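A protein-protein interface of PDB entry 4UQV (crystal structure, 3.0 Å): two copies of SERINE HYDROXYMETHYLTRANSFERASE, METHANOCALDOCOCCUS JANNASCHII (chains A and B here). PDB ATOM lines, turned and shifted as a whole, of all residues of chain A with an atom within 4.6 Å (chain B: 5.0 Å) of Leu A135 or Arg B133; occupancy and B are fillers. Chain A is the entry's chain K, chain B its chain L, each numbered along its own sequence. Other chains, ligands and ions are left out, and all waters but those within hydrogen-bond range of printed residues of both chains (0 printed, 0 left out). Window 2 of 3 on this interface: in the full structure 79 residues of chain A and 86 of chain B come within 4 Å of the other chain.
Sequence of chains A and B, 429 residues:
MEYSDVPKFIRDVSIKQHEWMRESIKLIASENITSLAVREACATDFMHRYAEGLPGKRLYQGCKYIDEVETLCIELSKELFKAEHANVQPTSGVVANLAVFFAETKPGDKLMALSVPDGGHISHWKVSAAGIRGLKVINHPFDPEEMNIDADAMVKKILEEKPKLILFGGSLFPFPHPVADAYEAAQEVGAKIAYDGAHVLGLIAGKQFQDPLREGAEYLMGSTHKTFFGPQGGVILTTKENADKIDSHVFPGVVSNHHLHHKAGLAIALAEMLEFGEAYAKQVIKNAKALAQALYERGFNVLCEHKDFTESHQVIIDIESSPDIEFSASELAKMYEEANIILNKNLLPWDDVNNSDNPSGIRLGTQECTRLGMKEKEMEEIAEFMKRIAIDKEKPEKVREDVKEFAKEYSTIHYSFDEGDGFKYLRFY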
ATOM      1  N   LYS A 126      23.210  -3.519   5.916  1.00  0.00           N
ATOM      2  CA  LYS A 126      21.773  -3.780   5.866  1.00  0.00           C
ATOM      3  C   LYS A 126      21.103  -3.774   7.236  1.00  0.00           C
ATOM      4  O   LYS A 126      21.771  -3.867   8.266  1.00  0.00           O
ATOM      5  CB  LYS A 126      21.508  -5.115   5.177  1.00  0.00           C
ATOM      6  CG  LYS A 126      22.034  -5.165   3.768  1.00  0.00           C
ATOM      7  CD  LYS A 126      21.213  -4.278   2.863  1.00  0.00           C
ATOM      8  CE  LYS A 126      20.109  -5.060   2.200  1.00  0.00           C
ATOM      9  NZ  LYS A 126      20.661  -5.942   1.134  1.00  0.00           N
ATOM     10  N   ALA A 130      20.968   3.031   4.054  1.00  0.00           N
ATOM     11  CA  ALA A 130      21.527   2.515   2.796  1.00  0.00           C
ATOM     12  C   ALA A 130      21.487   0.991   2.718  1.00  0.00           C
ATOM     13  O   ALA A 130      21.803   0.408   1.683  1.00  0.00           O
ATOM     14  CB  ALA A 130      22.974   2.960   2.602  1.00  0.00           C
ATOM     15  N   GLY A 131      21.107   0.344   3.813  1.00  0.00           N
ATOM     16  CA  GLY A 131      20.653  -1.028   3.762  1.00  0.00           C
ATOM     17  C   GLY A 131      19.181  -0.913   3.445  1.00  0.00           C
ATOM     18  O   GLY A 131      18.581  -1.769   2.795  1.00  0.00           O
ATOM     19  N   ILE A 132      18.608   0.183   3.927  1.00  0.00           N
ATOM     20  CA  ILE A 132      17.252   0.581   3.596  1.00  0.00           C
ATOM     21  C   ILE A 132      17.223   1.288   2.240  1.00  0.00           C
ATOM     22  O   ILE A 132      16.227   1.238   1.526  1.00  0.00           O
ATOM     23  CB  ILE A 132      16.667   1.494   4.692  1.00  0.00           C
ATOM     24  CG1 ILE A 132      16.765   0.805   6.054  1.00  0.00           C
ATOM     25  CG2 ILE A 132      15.217   1.841   4.394  1.00  0.00           C
ATOM     26  CD1 ILE A 132      16.664   1.746   7.226  1.00  0.00           C
ATOM     27  N   ARG A 133      18.328   1.929   1.872  1.00  0.00           N
ATOM     28  CA  ARG A 133      18.370   2.678   0.617  1.00  0.00           C
ATOM     29  C   ARG A 133      19.309   2.081  -0.426  1.00  0.00           C
ATOM     30  O   ARG A 133      18.864   1.473  -1.399  1.00  0.00           O
ATOM     31  CB  ARG A 133      18.775   4.130   0.885  1.00  0.00           C
ATOM     32  CG  ARG A 133      19.045   4.954  -0.370  1.00  0.00           C
ATOM     33  CD  ARG A 133      17.847   5.004  -1.310  1.00  0.00           C
ATOM     34  NE  ARG A 133      18.185   5.699  -2.550  1.00  0.00           N
ATOM     35  CZ  ARG A 133      17.322   5.968  -3.524  1.00  0.00           C
ATOM     36  NH1 ARG A 133      16.052   5.604  -3.411  1.00  0.00           N
ATOM     37  NH2 ARG A 133      17.732   6.605  -4.613  1.00  0.00           N
ATOM     38  N   GLY A 134      20.608   2.256  -0.209  1.00  0.00           N
ATOM     39  CA  GLY A 134      21.608   1.967  -1.216  1.00  0.00           C
ATOM     40  C   GLY A 134      21.736   0.494  -1.533  1.00  0.00           C
ATOM     41  O   GLY A 134      22.153   0.142  -2.636  1.00  0.00           O
ATOM     42  N   LEU A 135      21.371  -0.358  -0.574  1.00  0.00           N
ATOM     43  CA  LEU A 135      21.611  -1.796  -0.653  1.00  0.00           C
ATOM     44  C   LEU A 135      23.119  -2.017  -0.767  1.00  0.00           C
ATOM     45  O   LEU A 135      23.895  -1.312  -0.123  1.00  0.00           O
ATOM     46  CB  LEU A 135      20.867  -2.389  -1.857  1.00  0.00           C
ATOM     47  CG  LEU A 135      20.224  -3.775  -1.857  1.00  0.00           C
ATOM     48  CD1 LEU A 135      19.073  -3.838  -0.883  1.00  0.00           C
ATOM     49  CD2 LEU A 135      19.729  -4.102  -3.252  1.00  0.00           C
ATOM     50  N   LYS A 136      23.516  -3.001  -1.572  1.00  0.00           N
ATOM     51  CA  LYS A 136      24.819  -3.028  -2.249  1.00  0.00           C
ATOM     52  C   LYS A 136      26.034  -2.529  -1.456  1.00  0.00           C
ATOM     53  O   LYS A 136      26.578  -1.473  -1.777  1.00  0.00           O
ATOM     54  CB  LYS A 136      24.731  -2.206  -3.530  1.00  0.00           C
ATOM     55  CG  LYS A 136      23.381  -2.231  -4.241  1.00  0.00           C
ATOM     56  CD  LYS A 136      23.099  -3.554  -4.923  1.00  0.00           C
ATOM     57  CE  LYS A 136      21.942  -3.417  -5.903  1.00  0.00           C
ATOM     58  NZ  LYS A 136      21.547  -4.727  -6.494  1.00  0.00           N
ATOM     59  N   VAL A 137      26.476  -3.268  -0.446  1.00  0.00           N
ATOM     60  CA  VAL A 137      27.547  -2.766   0.417  1.00  0.00           C
ATOM     61  C   VAL A 137      28.864  -3.526   0.225  1.00  0.00           C
ATOM     62  O   VAL A 137      28.870  -4.689  -0.179  1.00  0.00           O
ATOM     63  CB  VAL A 137      27.132  -2.834   1.903  1.00  0.00           C
ATOM     64  CG1 VAL A 137      27.147  -4.269   2.386  1.00  0.00           C
ATOM     65  CG2 VAL A 137      28.042  -1.961   2.768  1.00  0.00           C
ATOM     66  N   PHE B 102      10.123  -0.772   5.845  1.00  0.00           N
ATOM     67  CA  PHE B 102      11.264  -1.662   5.694  1.00  0.00           C
ATOM     68  C   PHE B 102      10.967  -3.039   6.277  1.00  0.00           C
ATOM     69  O   PHE B 102      11.572  -4.034   5.872  1.00  0.00           O
ATOM     70  CB  PHE B 102      12.499  -1.048   6.363  1.00  0.00           C
ATOM     71  CG  PHE B 102      13.709  -1.936   6.343  1.00  0.00           C
ATOM     72  CD1 PHE B 102      14.140  -2.519   5.163  1.00  0.00           C
ATOM     73  CD2 PHE B 102      14.427  -2.171   7.503  1.00  0.00           C
ATOM     74  CE1 PHE B 102      15.254  -3.333   5.144  1.00  0.00           C
ATOM     75  CE2 PHE B 102      15.545  -2.981   7.491  1.00  0.00           C
ATOM     76  CZ  PHE B 102      15.959  -3.563   6.310  1.00  0.00           C
ATOM     77  N   LYS B 106       9.858  -5.292  -0.288  1.00  0.00           N
ATOM     78  CA  LYS B 106      11.081  -5.317  -1.077  1.00  0.00           C
ATOM     79  C   LYS B 106      10.972  -4.169  -2.072  1.00  0.00           C
ATOM     80  O   LYS B 106       9.875  -3.655  -2.289  1.00  0.00           O
ATOM     81  CB  LYS B 106      11.251  -6.657  -1.801  1.00  0.00           C
ATOM     82  CG  LYS B 106      10.822  -7.879  -0.995  1.00  0.00           C
ATOM     83  CD  LYS B 106      10.281  -8.973  -1.911  1.00  0.00           C
ATOM     84  CE  LYS B 106       9.717 -10.151  -1.124  1.00  0.00           C
ATOM     85  NZ  LYS B 106      10.770 -10.943  -0.422  1.00  0.00           N
ATOM     86  N   PRO B 107      12.096  -3.742  -2.669  1.00  0.00           N
ATOM     87  CA  PRO B 107      11.942  -2.734  -3.722  1.00  0.00           C
ATOM     88  C   PRO B 107      11.091  -3.260  -4.877  1.00  0.00           C
ATOM     89  O   PRO B 107      11.380  -4.327  -5.419  1.00  0.00           O
ATOM     90  CB  PRO B 107      13.381  -2.474  -4.176  1.00  0.00           C
ATOM     91  CG  PRO B 107      14.220  -2.844  -2.999  1.00  0.00           C
ATOM     92  CD  PRO B 107      13.509  -3.987  -2.332  1.00  0.00           C
ATOM     93  N   GLY B 108      10.060  -2.508  -5.250  1.00  0.00           N
ATOM     94  CA  GLY B 108       9.140  -2.937  -6.289  1.00  0.00           C
ATOM     95  C   GLY B 108       7.805  -3.428  -5.755  1.00  0.00           C
ATOM     96  O   GLY B 108       6.853  -3.595  -6.518  1.00  0.00           O
ATOM     97  N   GLY B 131      10.191   6.151  -0.924  1.00  0.00           N
ATOM     98  CA  GLY B 131      10.831   5.893  -2.199  1.00  0.00           C
ATOM     99  C   GLY B 131      12.238   5.391  -1.953  1.00  0.00           C
ATOM    100  O   GLY B 131      13.065   5.323  -2.862  1.00  0.00           O
ATOM    101  N   ILE B 132      12.500   5.038  -0.701  1.00  0.00           N
ATOM    102  CA  ILE B 132      13.832   4.645  -0.270  1.00  0.00           C
ATOM    103  C   ILE B 132      14.081   3.155  -0.499  1.00  0.00           C
ATOM    104  O   ILE B 132      14.942   2.786  -1.298  1.00  0.00           O
ATOM    105  CB  ILE B 132      14.050   5.001   1.214  1.00  0.00           C
ATOM    106  CG1 ILE B 132      13.967   6.520   1.402  1.00  0.00           C
ATOM    107  CG2 ILE B 132      15.384   4.482   1.705  1.00  0.00           C
ATOM    108  CD1 ILE B 132      14.305   6.996   2.800  1.00  0.00           C
ATOM    109  N   ARG B 133      13.329   2.303   0.195  1.00  0.00           N
ATOM    110  CA  ARG B 133      13.483   0.857   0.048  1.00  0.00           C
ATOM    111  C   ARG B 133      12.459   0.271  -0.922  1.00  0.00           C
ATOM    112  O   ARG B 133      12.803  -0.116  -2.039  1.00  0.00           O
ATOM    113  CB  ARG B 133      13.373   0.166   1.412  1.00  0.00           C
ATOM    114  CG  ARG B 133      13.574  -1.347   1.380  1.00  0.00           C
ATOM    115  CD  ARG B 133      14.674  -1.772   0.409  1.00  0.00           C
ATOM    116  NE  ARG B 133      16.012  -1.338   0.802  1.00  0.00           N
ATOM    117  CZ  ARG B 133      17.035  -1.237  -0.043  1.00  0.00           C
ATOM    118  NH1 ARG B 133      16.862  -1.522  -1.327  1.00  0.00           N
ATOM    119  NH2 ARG B 133      18.227  -0.843   0.385  1.00  0.00           N
ATOM    120  N   GLY B 134      11.204   0.202  -0.492  1.00  0.00           N
ATOM    121  CA  GLY B 134      10.140  -0.280  -1.351  1.00  0.00           C
ATOM    122  C   GLY B 134       9.621   0.855  -2.207  1.00  0.00           C
ATOM    123  O   GLY B 134       9.666   2.010  -1.795  1.00  0.00           O
ATOM    124  N   LEU B 135       9.138   0.540  -3.404  1.00  0.00           N
ATOM    125  CA  LEU B 135       8.647   1.576  -4.308  1.00  0.00           C
ATOM    126  C   LEU B 135       7.356   1.150  -4.998  1.00  0.00           C
ATOM    127  O   LEU B 135       6.783   0.114  -4.665  1.00  0.00           O
ATOM    128  CB  LEU B 135       9.710   1.936  -5.350  1.00  0.00           C
ATOM    129  CG  LEU B 135      10.821   2.910  -4.933  1.00  0.00           C
ATOM    130  CD1 LEU B 135      11.919   2.219  -4.139  1.00  0.00           C
ATOM    131  CD2 LEU B 135      11.406   3.607  -6.151  1.00  0.00           C
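The backbone carbonyl oxygen (O) of Arg A133 sits at hydrogen-bond distance from the guanidinium group (NH2) of Arg B133 (3.0 Å).
The backbone carbonyl oxygen (O) of Gly A131 is in hydrogen-bond range of the guanidinium group (NH2) of Arg B133 (2.6 Å).
The backbone NH (N) of Leu A135 sits close to the guanidinium group (NH2) of Arg B133, 3.3 Å away.
The guanidinium group (NE) of Arg B133 sits at hydrogen-bond distance from the backbone carbonyl oxygen (O) of Ile A132.
O of Ile A132 lies close to O of Ile B132 (3.5 Å).
NH1 of Arg A133 is in hydrogen-bond range of O of Gly B131, at 3.1 Å.
The backbone carbonyl oxygen (O) of Ala A130 lies within hydrogen-bond range of the backbone NH (N) of Leu A135 (2.4 Å).
Arg A133 touches Ile B132.
Gly A134 touches Arg B133 (N to NH2, 3.95 Å).
Of the printed residues of chain B, Gly A131 touches Arg B133 (2.6 Å).
Of the printed residues of chain B, Ile A132 touches Ile B132 (3.4 Å) and Arg B133 (2.7 Å).
Printed residues of chain B within 4 Å of Arg A133: Gly B131, Ile B132 and Arg B133.
Leu A135 touches one residue of chain B.
Lys B106 touches none of the printed residues of chain A.
Of the printed residues of chain A, Gly B131 touches Arg A133.
Printed residues of chain A within 4 Å of Ile B132: Ile A132 and Arg A133.
Of the printed residues of chain A, Arg B133 touches Gly A131, Ile A132, Arg A133, Gly A134 and Leu A135.
Leu B135 touches none of the printed residues of chain A.
The nearest printed residue of chain A that does not touch Arg B133 is Ala A130 (4.005 Å).
The nearest printed residue of chain A that does not touch Gly B131 is Ile A132 (6.7 Å).
Printed residues of chain B that touch a printed residue of chain A: Gly B131, Ile B132 and Arg B133.
Of the 9 printed residues of chain A, 5 touch a printed residue of chain B.
Printed residues of chain A that touch a printed residue of chain B: Gly A131, Ile A132, Arg A133, Gly A134 and Leu A135.
Among the printed residues, 8 pairs touch across the chains.
Among the printed residues, no Asp or Glu carboxylate lies within 4 Å of a Lys or Arg side-chain nitrogen of the other chain.
Gly A131 touches Arg B133, and with the chains exchanged Arg A133 touches Gly B131.
Ile A132 touches Arg B133, and with the chains exchanged Arg A133 touches Ile B132.
Arg A133 touches its own counterpart, Arg B133.
Gly A134 touches Arg B133, but with the chains exchanged Arg A133 does not touch Gly B134 (7.5 Å).
Positions printed for both chains: 131, 132, 133, 134 and 135.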
